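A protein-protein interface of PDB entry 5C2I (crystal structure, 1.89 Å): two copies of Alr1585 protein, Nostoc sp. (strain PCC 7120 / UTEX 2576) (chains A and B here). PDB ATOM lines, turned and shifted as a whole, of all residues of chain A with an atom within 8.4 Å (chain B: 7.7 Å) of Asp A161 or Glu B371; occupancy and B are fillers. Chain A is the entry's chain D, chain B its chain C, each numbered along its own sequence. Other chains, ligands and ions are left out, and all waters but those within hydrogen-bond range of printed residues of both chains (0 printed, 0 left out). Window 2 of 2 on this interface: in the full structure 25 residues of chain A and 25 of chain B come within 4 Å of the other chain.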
ATOM      1  N   VAL A  44      -0.229   4.293   5.353  1.00  0.00           N
ATOM      2  CA  VAL A  44      -1.375   5.032   4.857  1.00  0.00           C
ATOM      3  C   VAL A  44      -1.130   6.504   5.181  1.00  0.00           C
ATOM      4  O   VAL A  44      -0.769   6.866   6.309  1.00  0.00           O
ATOM      5  CB  VAL A  44      -2.703   4.553   5.468  1.00  0.00           C
ATOM      6  CG1 VAL A  44      -3.870   5.425   4.990  1.00  0.00           C
ATOM      7  CG2 VAL A  44      -2.962   3.094   5.134  1.00  0.00           C
ATOM      8  N   VAL A  92       0.485  -0.193  15.894  1.00  0.00           N
ATOM      9  CA  VAL A  92       0.724   0.559  14.676  1.00  0.00           C
ATOM     10  C   VAL A  92       1.626   1.759  14.973  1.00  0.00           C
ATOM     11  O   VAL A  92       1.634   2.281  16.093  1.00  0.00           O
ATOM     12  CB  VAL A  92      -0.547   1.129  13.987  1.00  0.00           C
ATOM     13  CG1 VAL A  92      -1.365   0.015  13.401  1.00  0.00           C
ATOM     14  CG2 VAL A  92      -1.397   1.974  14.900  1.00  0.00           C
ATOM     15  N   ILE A 154       0.031   6.517   9.163  1.00  0.00           N
ATOM     16  CA  ILE A 154      -0.119   5.297   9.962  1.00  0.00           C
ATOM     17  C   ILE A 154       0.575   4.191   9.205  1.00  0.00           C
ATOM     18  O   ILE A 154       0.398   4.063   8.005  1.00  0.00           O
ATOM     19  CB  ILE A 154      -1.599   4.885  10.185  1.00  0.00           C
ATOM     20  CG1 ILE A 154      -2.376   6.066  10.775  1.00  0.00           C
ATOM     21  CG2 ILE A 154      -1.717   3.749  11.183  1.00  0.00           C
ATOM     22  CD1 ILE A 154      -3.163   6.808   9.729  1.00  0.00           C
ATOM     23  N   ALA A 155       1.357   3.393   9.915  1.00  0.00           N
ATOM     24  CA  ALA A 155       2.181   2.386   9.295  1.00  0.00           C
ATOM     25  C   ALA A 155       2.252   1.095  10.130  1.00  0.00           C
ATOM     26  O   ALA A 155       2.161   1.102  11.335  1.00  0.00           O
ATOM     27  CB  ALA A 155       3.581   2.938   9.027  1.00  0.00           C
ATOM     28  N   ASP A 156       2.387  -0.013   9.423  1.00  0.00           N
ATOM     29  CA  ASP A 156       2.424  -1.328  10.029  1.00  0.00           C
ATOM     30  C   ASP A 156       2.941  -2.331   9.005  1.00  0.00           C
ATOM     31  O   ASP A 156       2.736  -2.139   7.805  1.00  0.00           O
ATOM     32  CB  ASP A 156       1.047  -1.760  10.498  1.00  0.00           C
ATOM     33  CG  ASP A 156       1.131  -2.790  11.607  1.00  0.00           C
ATOM     34  OD1 ASP A 156       1.236  -2.393  12.780  1.00  0.00           O
ATOM     35  OD2 ASP A 156       1.142  -4.001  11.326  1.00  0.00           O
ATOM     36  N   ASP A 157       3.591  -3.408   9.460  1.00  0.00           N
ATOM     37  CA  ASP A 157       3.957  -4.501   8.544  1.00  0.00           C
ATOM     38  C   ASP A 157       2.764  -5.380   8.079  1.00  0.00           C
ATOM     39  O   ASP A 157       2.844  -5.980   7.004  1.00  0.00           O
ATOM     40  CB  ASP A 157       5.007  -5.417   9.198  1.00  0.00           C
ATOM     41  CG  ASP A 157       6.362  -4.716   9.368  1.00  0.00           C
ATOM     42  OD1 ASP A 157       6.743  -3.876   8.561  1.00  0.00           O
ATOM     43  OD2 ASP A 157       7.021  -5.017  10.348  1.00  0.00           O
ATOM     44  N   ASP A 158       1.713  -5.479   8.886  1.00  0.00           N
ATOM     45  CA  ASP A 158       0.550  -6.321   8.589  1.00  0.00           C
ATOM     46  C   ASP A 158      -0.455  -5.431   7.838  1.00  0.00           C
ATOM     47  O   ASP A 158      -1.143  -4.617   8.443  1.00  0.00           O
ATOM     48  CB  ASP A 158      -0.045  -6.885   9.893  1.00  0.00           C
ATOM     49  CG  ASP A 158      -1.317  -7.747   9.682  1.00  0.00           C
ATOM     50  OD1 ASP A 158      -2.025  -7.647   8.640  1.00  0.00           O
ATOM     51  OD2 ASP A 158      -1.660  -8.530  10.612  1.00  0.00           O
ATOM     52  N   ILE A 159      -0.507  -5.567   6.509  1.00  0.00           N
ATOM     53  CA  ILE A 159      -1.351  -4.655   5.702  1.00  0.00           C
ATOM     54  C   ILE A 159      -2.834  -4.759   6.077  1.00  0.00           C
ATOM     55  O   ILE A 159      -3.499  -3.747   6.248  1.00  0.00           O
ATOM     56  CB  ILE A 159      -1.080  -4.818   4.186  1.00  0.00           C
ATOM     57  CG1 ILE A 159      -1.872  -3.816   3.343  1.00  0.00           C
ATOM     58  CG2 ILE A 159      -1.417  -6.214   3.682  1.00  0.00           C
ATOM     59  CD1 ILE A 159      -1.705  -2.362   3.722  1.00  0.00           C
ATOM     60  N   VAL A 160      -3.372  -5.963   6.225  1.00  0.00           N
ATOM     61  CA  VAL A 160      -4.801  -6.090   6.477  1.00  0.00           C
ATOM     62  C   VAL A 160      -5.155  -5.403   7.800  1.00  0.00           C
ATOM     63  O   VAL A 160      -6.121  -4.635   7.879  1.00  0.00           O
ATOM     64  CB  VAL A 160      -5.249  -7.557   6.466  1.00  0.00           C
ATOM     65  CG1 VAL A 160      -6.672  -7.693   6.990  1.00  0.00           C
ATOM     66  CG2 VAL A 160      -5.122  -8.145   5.062  1.00  0.00           C
ATOM     67  N   ASP A 161      -4.349  -5.632   8.838  1.00  0.00           N
ATOM     68  CA  ASP A 161      -4.601  -5.004  10.151  1.00  0.00           C
ATOM     69  C   ASP A 161      -4.453  -3.478  10.072  1.00  0.00           C
ATOM     70  O   ASP A 161      -5.283  -2.754  10.631  1.00  0.00           O
ATOM     71  CB  ASP A 161      -3.833  -5.709  11.278  1.00  0.00           C
ATOM     72  CG  ASP A 161      -4.595  -6.872  11.901  1.00  0.00           C
ATOM     73  OD1 ASP A 161      -5.805  -7.280  11.567  1.00  0.00           O
ATOM     74  OD2 ASP A 161      -3.858  -7.469  12.730  1.00  0.00           O
ATOM     75  N   LEU A 162      -3.473  -2.996   9.334  1.00  0.00           N
ATOM     76  CA  LEU A 162      -3.315  -1.579   9.093  1.00  0.00           C
ATOM     77  C   LEU A 162      -4.597  -0.964   8.518  1.00  0.00           C
ATOM     78  O   LEU A 162      -5.054   0.100   8.977  1.00  0.00           O
ATOM     79  CB  LEU A 162      -2.160  -1.314   8.131  1.00  0.00           C
ATOM     80  CG  LEU A 162      -1.934   0.112   7.692  1.00  0.00           C
ATOM     81  CD1 LEU A 162      -1.718   1.070   8.881  1.00  0.00           C
ATOM     82  CD2 LEU A 162      -0.767   0.240   6.703  1.00  0.00           C
ATOM     83  N   LEU A 163      -5.157  -1.627   7.514  1.00  0.00           N
ATOM     84  CA  LEU A 163      -6.376  -1.114   6.864  1.00  0.00           C
ATOM     85  C   LEU A 163      -7.511  -1.029   7.857  1.00  0.00           C
ATOM     86  O   LEU A 163      -8.306  -0.060   7.837  1.00  0.00           O
ATOM     87  CB  LEU A 163      -6.765  -1.981   5.677  1.00  0.00           C
ATOM     88  CG  LEU A 163      -5.720  -2.021   4.573  1.00  0.00           C
ATOM     89  CD1 LEU A 163      -6.088  -3.077   3.521  1.00  0.00           C
ATOM     90  CD2 LEU A 163      -5.495  -0.673   3.913  1.00  0.00           C
ATOM     91  N   GLN A 164      -7.656  -2.051   8.704  1.00  0.00           N
ATOM     92  CA  GLN A 164      -8.755  -2.068   9.668  1.00  0.00           C
ATOM     93  C   GLN A 164      -8.612  -0.922  10.670  1.00  0.00           C
ATOM     94  O   GLN A 164      -9.605  -0.248  11.044  1.00  0.00           O
ATOM     95  CB  GLN A 164      -8.840  -3.392  10.436  1.00  0.00           C
ATOM     96  CG  GLN A 164      -8.837  -4.655   9.577  1.00  0.00           C
ATOM     97  CD  GLN A 164      -9.881  -4.641   8.459  1.00  0.00           C
ATOM     98  OE1 GLN A 164     -11.087  -4.603   8.730  1.00  0.00           O
ATOM     99  NE2 GLN A 164      -9.426  -4.741   7.223  1.00  0.00           N
ATOM    100  N   ILE A 165      -7.394  -0.730  11.131  1.00  0.00           N
ATOM    101  CA  ILE A 165      -7.148   0.296  12.147  1.00  0.00           C
ATOM    102  C   ILE A 165      -7.393   1.681  11.543  1.00  0.00           C
ATOM    103  O   ILE A 165      -8.005   2.526  12.168  1.00  0.00           O
ATOM    104  CB  ILE A 165      -5.718   0.153  12.716  1.00  0.00           C
ATOM    105  CG1 ILE A 165      -5.672  -1.082  13.600  1.00  0.00           C
ATOM    106  CG2 ILE A 165      -5.333   1.377  13.523  1.00  0.00           C
ATOM    107  CD1 ILE A 165      -4.256  -1.526  13.961  1.00  0.00           C
ATOM    108  N   VAL A 166      -6.941   1.897  10.330  1.00  0.00           N
ATOM    109  CA  VAL A 166      -7.226   3.136   9.637  1.00  0.00           C
ATOM    110  C   VAL A 166      -8.734   3.361   9.515  1.00  0.00           C
ATOM    111  O   VAL A 166      -9.224   4.466   9.768  1.00  0.00           O
ATOM    112  CB  VAL A 166      -6.536   3.194   8.262  1.00  0.00           C
ATOM    113  CG1 VAL A 166      -7.089   4.326   7.426  1.00  0.00           C
ATOM    114  CG2 VAL A 166      -5.051   3.370   8.438  1.00  0.00           C
ATOM    115  N   ASN A 167      -9.485   2.335   9.128  1.00  0.00           N
ATOM    116  CA  ASN A 167     -10.937   2.508   8.970  1.00  0.00           C
ATOM    117  C   ASN A 167     -11.589   2.862  10.298  1.00  0.00           C
ATOM    118  O   ASN A 167     -12.579   3.598  10.327  1.00  0.00           O
ATOM    119  CB  ASN A 167     -11.579   1.267   8.362  1.00  0.00           C
ATOM    120  CG  ASN A 167     -11.190   1.089   6.908  1.00  0.00           C
ATOM    121  OD1 ASN A 167     -10.772   2.049   6.251  1.00  0.00           O
ATOM    122  ND2 ASN A 167     -11.318  -0.114   6.405  1.00  0.00           N
ATOM    123  N   GLN A 168     -11.047   2.346  11.391  1.00  0.00           N
ATOM    124  CA  GLN A 168     -11.548   2.701  12.713  1.00  0.00           C
ATOM    125  C   GLN A 168     -11.238   4.151  13.027  1.00  0.00           C
ATOM    126  O   GLN A 168     -12.112   4.914  13.428  1.00  0.00           O
ATOM    127  CB  GLN A 168     -10.944   1.782  13.761  1.00  0.00           C
ATOM    128  CG  GLN A 168     -11.490   2.008  15.162  1.00  0.00           C
ATOM    129  CD  GLN A 168     -10.995   0.940  16.137  1.00  0.00           C
ATOM    130  OE1 GLN A 168     -10.523  -0.131  15.739  1.00  0.00           O
ATOM    131  NE2 GLN A 168     -11.054   1.256  17.415  1.00  0.00           N
ATOM    132  N   ILE A 169      -9.990   4.541  12.848  1.00  0.00           N
ATOM    133  CA  ILE A 169      -9.553   5.929  13.098  1.00  0.00           C
ATOM    134  C   ILE A 169     -10.361   6.946  12.294  1.00  0.00           C
ATOM    135  O   ILE A 169     -10.767   7.966  12.838  1.00  0.00           O
ATOM    136  CB  ILE A 169      -8.036   6.086  12.784  1.00  0.00           C
ATOM    137  CG1 ILE A 169      -7.196   5.347  13.847  1.00  0.00           C
ATOM    138  CG2 ILE A 169      -7.648   7.553  12.649  1.00  0.00           C
ATOM    139  CD1 ILE A 169      -5.754   5.122  13.418  1.00  0.00           C
ATOM    140  N   PHE B 186     -11.758  -8.892   3.904  1.00  0.00           N
ATOM    141  CA  PHE B 186     -10.821  -9.956   3.603  1.00  0.00           C
ATOM    142  C   PHE B 186     -11.433 -11.329   3.930  1.00  0.00           C
ATOM    143  O   PHE B 186     -12.482 -11.420   4.581  1.00  0.00           O
ATOM    144  CB  PHE B 186      -9.537  -9.762   4.371  1.00  0.00           C
ATOM    145  CG  PHE B 186      -9.696  -9.773   5.843  1.00  0.00           C
ATOM    146  CD1 PHE B 186      -9.997  -8.603   6.537  1.00  0.00           C
ATOM    147  CD2 PHE B 186      -9.564 -10.952   6.555  1.00  0.00           C
ATOM    148  CE1 PHE B 186     -10.126  -8.597   7.881  1.00  0.00           C
ATOM    149  CE2 PHE B 186      -9.707 -10.953   7.933  1.00  0.00           C
ATOM    150  CZ  PHE B 186     -10.017  -9.771   8.587  1.00  0.00           C
ATOM    151  N   LEU B 188     -11.039 -14.765   5.886  1.00  0.00           N
ATOM    152  CA  LEU B 188     -10.410 -15.551   6.942  1.00  0.00           C
ATOM    153  C   LEU B 188     -10.350 -16.996   6.569  1.00  0.00           C
ATOM    154  O   LEU B 188     -11.333 -17.524   6.044  1.00  0.00           O
ATOM    155  CB  LEU B 188     -11.246 -15.492   8.252  1.00  0.00           C
ATOM    156  CG  LEU B 188     -10.999 -14.483   9.313  1.00  0.00           C
ATOM    157  CD1 LEU B 188     -11.906 -14.790  10.496  1.00  0.00           C
ATOM    158  CD2 LEU B 188      -9.549 -14.472   9.753  1.00  0.00           C
ATOM    159  N   HIS B 198     -15.226 -15.497  12.013  1.00  0.00           N
ATOM    160  CA  HIS B 198     -14.402 -15.241  13.203  1.00  0.00           C
ATOM    161  C   HIS B 198     -14.576 -16.203  14.369  1.00  0.00           C
ATOM    162  O   HIS B 198     -13.657 -16.367  15.158  1.00  0.00           O
ATOM    163  CB  HIS B 198     -14.648 -13.813  13.714  1.00  0.00           C
ATOM    164  CG  HIS B 198     -13.852 -12.782  12.992  1.00  0.00           C
ATOM    165  ND1 HIS B 198     -12.526 -12.587  13.279  1.00  0.00           N
ATOM    166  CD2 HIS B 198     -14.171 -11.883  12.033  1.00  0.00           C
ATOM    167  CE1 HIS B 198     -12.036 -11.644  12.492  1.00  0.00           C
ATOM    168  NE2 HIS B 198     -13.020 -11.188  11.741  1.00  0.00           N
ATOM    169  N   VAL B 263     -15.715 -12.628  19.829  1.00  0.00           N
ATOM    170  CA  VAL B 263     -15.128 -13.957  19.759  1.00  0.00           C
ATOM    171  C   VAL B 263     -14.737 -14.457  21.136  1.00  0.00           C
ATOM    172  O   VAL B 263     -15.035 -15.608  21.511  1.00  0.00           O
ATOM    173  CB  VAL B 263     -13.910 -13.958  18.846  1.00  0.00           C
ATOM    174  CG1 VAL B 263     -13.261 -15.337  18.810  1.00  0.00           C
ATOM    175  CG2 VAL B 263     -14.290 -13.533  17.436  1.00  0.00           C
ATOM    176  N   SER B 368     -15.041 -10.807   5.758  1.00  0.00           N
ATOM    177  CA  SER B 368     -14.720 -10.499   7.138  1.00  0.00           C
ATOM    178  C   SER B 368     -14.088  -9.105   7.270  1.00  0.00           C
ATOM    179  O   SER B 368     -13.536  -8.565   6.313  1.00  0.00           O
ATOM    180  CB  SER B 368     -13.757 -11.566   7.702  1.00  0.00           C
ATOM    181  OG  SER B 368     -14.503 -12.752   7.972  1.00  0.00           O
ATOM    182  N   TYR B 369     -14.200  -8.538   8.470  1.00  0.00           N
ATOM    183  CA  TYR B 369     -13.447  -7.337   8.856  1.00  0.00           C
ATOM    184  C   TYR B 369     -12.781  -7.485  10.202  1.00  0.00           C
ATOM    185  O   TYR B 369     -13.100  -8.379  10.986  1.00  0.00           O
ATOM    186  CB  TYR B 369     -14.358  -6.104   8.889  1.00  0.00           C
ATOM    187  CG  TYR B 369     -15.310  -6.013  10.054  1.00  0.00           C
ATOM    188  CD1 TYR B 369     -16.570  -6.589  10.009  1.00  0.00           C
ATOM    189  CD2 TYR B 369     -14.966  -5.288  11.197  1.00  0.00           C
ATOM    190  CE1 TYR B 369     -17.457  -6.443  11.096  1.00  0.00           C
ATOM    191  CE2 TYR B 369     -15.812  -5.162  12.263  1.00  0.00           C
ATOM    192  CZ  TYR B 369     -17.060  -5.751  12.208  1.00  0.00           C
ATOM    193  OH  TYR B 369     -17.900  -5.558  13.267  1.00  0.00           O
ATOM    194  N   GLY B 370     -11.837  -6.597  10.463  1.00  0.00           N
ATOM    195  CA  GLY B 370     -11.142  -6.551  11.750  1.00  0.00           C
ATOM    196  C   GLY B 370      -9.938  -7.480  11.832  1.00  0.00           C
ATOM    197  O   GLY B 370      -9.167  -7.572  10.910  1.00  0.00           O
ATOM    198  N   GLU B 371      -9.834  -8.206  12.933  1.00  0.00           N
ATOM    199  CA  GLU B 371      -8.640  -9.048  13.200  1.00  0.00           C
ATOM    200  C   GLU B 371      -8.465 -10.129  12.137  1.00  0.00           C
ATOM    201  O   GLU B 371      -9.395 -10.869  11.867  1.00  0.00           O
ATOM    202  CB  GLU B 371      -8.811  -9.733  14.555  1.00  0.00           C
ATOM    203  CG  GLU B 371      -7.685 -10.699  14.898  1.00  0.00           C
ATOM    204  CD  GLU B 371      -6.375  -9.966  14.955  1.00  0.00           C
ATOM    205  OE1 GLU B 371      -6.242  -9.162  15.888  1.00  0.00           O
ATOM    206  OE2 GLU B 371      -5.535 -10.175  14.042  1.00  0.00           O
ATOM    207  N   ASN B 372      -7.292 -10.206  11.534  1.00  0.00           N
ATOM    208  CA  ASN B 372      -7.065 -11.207  10.489  1.00  0.00           C
ATOM    209  C   ASN B 372      -6.344 -12.478  10.926  1.00  0.00           C
ATOM    210  O   ASN B 372      -6.278 -13.454  10.168  1.00  0.00           O
ATOM    211  CB  ASN B 372      -6.391 -10.577   9.276  1.00  0.00           C
ATOM    212  CG  ASN B 372      -4.907 -10.392   9.441  1.00  0.00           C
ATOM    213  OD1 ASN B 372      -4.163 -10.983   8.690  1.00  0.00           O
ATOM    214  ND2 ASN B 372      -4.479  -9.533  10.315  1.00  0.00           N
ATOM    215  N   ASN B 373      -5.825 -12.477  12.140  1.00  0.00           N
ATOM    216  CA  ASN B 373      -5.300 -13.699  12.724  1.00  0.00           C
ATOM    217  C   ASN B 373      -6.421 -14.502  13.434  1.00  0.00           C
ATOM    218  O   ASN B 373      -6.869 -14.094  14.507  1.00  0.00           O
ATOM    219  CB  ASN B 373      -4.193 -13.338  13.685  1.00  0.00           C
ATOM    220  CG  ASN B 373      -3.564 -14.548  14.316  1.00  0.00           C
ATOM    221  OD1 ASN B 373      -4.125 -15.655  14.274  1.00  0.00           O
ATOM    222  ND2 ASN B 373      -2.433 -14.334  14.963  1.00  0.00           N
ATOM    223  N   PRO B 374      -6.838 -15.667  12.862  1.00  0.00           N
ATOM    224  CA  PRO B 374      -8.007 -16.396  13.414  1.00  0.00           C
ATOM    225  C   PRO B 374      -7.733 -17.081  14.751  1.00  0.00           C
ATOM    226  O   PRO B 374      -8.682 -17.549  15.373  1.00  0.00           O
ATOM    227  CB  PRO B 374      -8.333 -17.439  12.329  1.00  0.00           C
ATOM    228  CG  PRO B 374      -7.010 -17.686  11.681  1.00  0.00           C
ATOM    229  CD  PRO B 374      -6.275 -16.368  11.688  1.00  0.00           C
ATOM    230  N   SER B 375      -6.486 -17.083  15.227  1.00  0.00           N
ATOM    231  CA  SER B 375      -6.204 -17.596  16.567  1.00  0.00           C
ATOM    232  C   SER B 375      -6.538 -16.597  17.671  1.00  0.00           C
ATOM    233  O   SER B 375      -6.627 -16.985  18.855  1.00  0.00           O
ATOM    234  CB  SER B 375      -4.731 -17.977  16.692  1.00  0.00           C
ATOM    235  OG  SER B 375      -3.959 -16.788  16.705  1.00  0.00           O
ATOM    236  N   LYS B 376      -6.688 -15.311  17.318  1.00  0.00           N
ATOM    237  CA  LYS B 376      -6.937 -14.283  18.339  1.00  0.00           C
ATOM    238  C   LYS B 376      -8.409 -14.221  18.675  1.00  0.00           C
ATOM    239  O   LYS B 376      -9.239 -14.808  17.980  1.00  0.00           O
ATOM    240  CB  LYS B 376      -6.435 -12.926  17.896  1.00  0.00           C
ATOM    241  CG  LYS B 376      -4.937 -12.870  17.831  1.00  0.00           C
ATOM    242  CD  LYS B 376      -4.531 -11.486  17.390  1.00  0.00           C
ATOM    243  CE  LYS B 376      -3.042 -11.358  17.145  1.00  0.00           C
ATOM    244  NZ  LYS B 376      -2.395 -10.713  18.301  1.00  0.00           N
ATOM    245  N   GLU B 377      -8.736 -13.538  19.767  1.00  0.00           N
ATOM    246  CA  GLU B 377     -10.102 -13.518  20.268  1.00  0.00           C
ATOM    247  C   GLU B 377     -10.530 -12.090  20.531  1.00  0.00           C
ATOM    248  O   GLU B 377     -10.637 -11.661  21.674  1.00  0.00           O
ATOM    249  CB  GLU B 377     -10.231 -14.427  21.493  1.00  0.00           C
ATOM    250  CG  GLU B 377     -10.092 -15.905  21.097  1.00  0.00           C
ATOM    251  CD  GLU B 377     -10.353 -16.883  22.241  1.00  0.00           C
ATOM    252  OE1 GLU B 377     -10.574 -16.463  23.395  1.00  0.00           O
ATOM    253  OE2 GLU B 377     -10.324 -18.102  21.946  1.00  0.00           O
ATOM    254  N   PRO B 378     -10.817 -11.340  19.467  1.00  0.00           N
ATOM    255  CA  PRO B 378     -11.276  -9.960  19.658  1.00  0.00           C
ATOM    256  C   PRO B 378     -12.620  -9.869  20.364  1.00  0.00           C
ATOM    257  O   PRO B 378     -13.511 -10.707  20.152  1.00  0.00           O
ATOM    258  CB  PRO B 378     -11.374  -9.430  18.231  1.00  0.00           C
ATOM    259  CG  PRO B 378     -11.626 -10.623  17.411  1.00  0.00           C
ATOM    260  CD  PRO B 378     -10.813 -11.718  18.048  1.00  0.00           C
ATOM    261  N   SER B 380     -14.256  -6.554  20.450  1.00  0.00           N
ATOM    262  CA  SER B 380     -14.971  -5.620  19.593  1.00  0.00           C
ATOM    263  C   SER B 380     -14.077  -5.266  18.417  1.00  0.00           C
ATOM    264  O   SER B 380     -12.864  -5.536  18.455  1.00  0.00           O
ATOM    265  CB  SER B 380     -15.372  -4.342  20.386  1.00  0.00           C
ATOM    266  OG  SER B 380     -14.214  -3.710  20.861  1.00  0.00           O
ATOM    267  N   GLY B 381     -14.672  -4.678  17.387  1.00  0.00           N
ATOM    268  CA  GLY B 381     -13.958  -4.222  16.201  1.00  0.00           C
ATOM    269  C   GLY B 381     -13.698  -5.280  15.140  1.00  0.00           C
ATOM    270  O   GLY B 381     -13.050  -4.977  14.112  1.00  0.00           O
ATOM    271  N   SER B 382     -14.205  -6.509  15.353  1.00  0.00           N
ATOM    272  CA  SER B 382     -14.073  -7.587  14.365  1.00  0.00           C
ATOM    273  C   SER B 382     -15.392  -8.272  14.092  1.00  0.00           C
ATOM    274  O   SER B 382     -16.222  -8.375  14.978  1.00  0.00           O
ATOM    275  CB  SER B 382     -13.097  -8.650  14.863  1.00  0.00           C
ATOM    276  OG  SER B 382     -11.755  -8.156  14.910  1.00  0.00           O
ATOM    277  N   GLY B 383     -15.567  -8.742  12.875  1.00  0.00           N
ATOM    278  CA  GLY B 383     -16.791  -9.447  12.525  1.00  0.00           C
ATOM    279  C   GLY B 383     -17.006  -9.756  11.079  1.00  0.00           C
ATOM    280  O   GLY B 383     -16.046  -9.951  10.319  1.00  0.00           O
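N of Tyr B369 is in hydrogen-bond range of O of Gly B383. The backbone NH of Ser B368 lies within hydrogen-bond range of the backbone carbonyl oxygen of Phe B186, at 2.9 Å. The side-chain carboxylate (OD1) of Asp A158 sits at hydrogen-bond distance from the backbone NH (N) of Val A160, at 3.2 Å. The backbone NH (N) of Asn B373 sits at hydrogen-bond distance from the side-chain carboxylate (OE2) of Glu B371 (3.0 Å). The backbone carbonyl oxygen (O) of Val A160 sits close to the side-chain amide nitrogen (NE2) of Gln A164 (3.4 Å). The backbone NH of Asp A161 lies within hydrogen-bond range of the side-chain carboxylate of Asp A158 (3.1 Å).
Asp A161 touches three residues of chain B. Of the printed residues of chain A, Glu B371 touches Asp A161 (3.4 Å). Gly B370 touches two residues of chain A. Of the printed residues of chain A, Phe B186 touches Val A160 (3.5 Å) and Gln A164 (3.96 Å). Of the printed residues of chain B, Asp A158 touches Asn B372. Of the printed residues of chain A, Tyr B369 touches Gln A164 (3.6 Å). Printed residues of chain B within 4 Å of Gln A164: Phe B186 (3.96 Å), Tyr B369 (3.6 Å) and Gly B370 (2.7 Å). The nearest printed residue of chain B that does not touch Asp A158 is Glu B371 (5.4 Å).
The side-chain carboxylate of Asp A161 lies close to the backbone carbonyl oxygen of Gly B370. ND2 of Asn B372 is in hydrogen-bond range of OD2 of Asp A158 (3.0 Å). OD2 of Asp A161 lies close to OE2 of Glu B371, at 3.4 Å. The side-chain amide nitrogen (ND2) of Asn B372 lies within hydrogen-bond range of the side-chain carboxylate (OD1) of Asp A161 (2.9 Å). The side-chain amide oxygen (OE1) of Gln A164 lies within hydrogen-bond range of the backbone NH (N) of Gly B370 (2.7 Å).
No position is printed for both chains.
CG1 of Val A160 touches CD1 of Phe B186 (3.5 Å). Asn B372 touches Val A160. Gln A164 touches Phe B186. Tyr B369 touches Gln A164 (CB to OE1, 3.6 Å).
Of the 18 printed residues of chain A, 4 touch a printed residue of chain B. Of the 19 printed residues of chain B, 5 touch a printed residue of chain A. Hydrophobic or aromatic side chains of chain B within 4 Å of the printed part of chain A: Phe B186 and Tyr B369. Among the printed residues, 9 pairs touch across the chains. Among the printed residues, no Asp or Glu carboxylate lies within 4 Å of a Lys or Arg side-chain nitrogen of the other chain.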
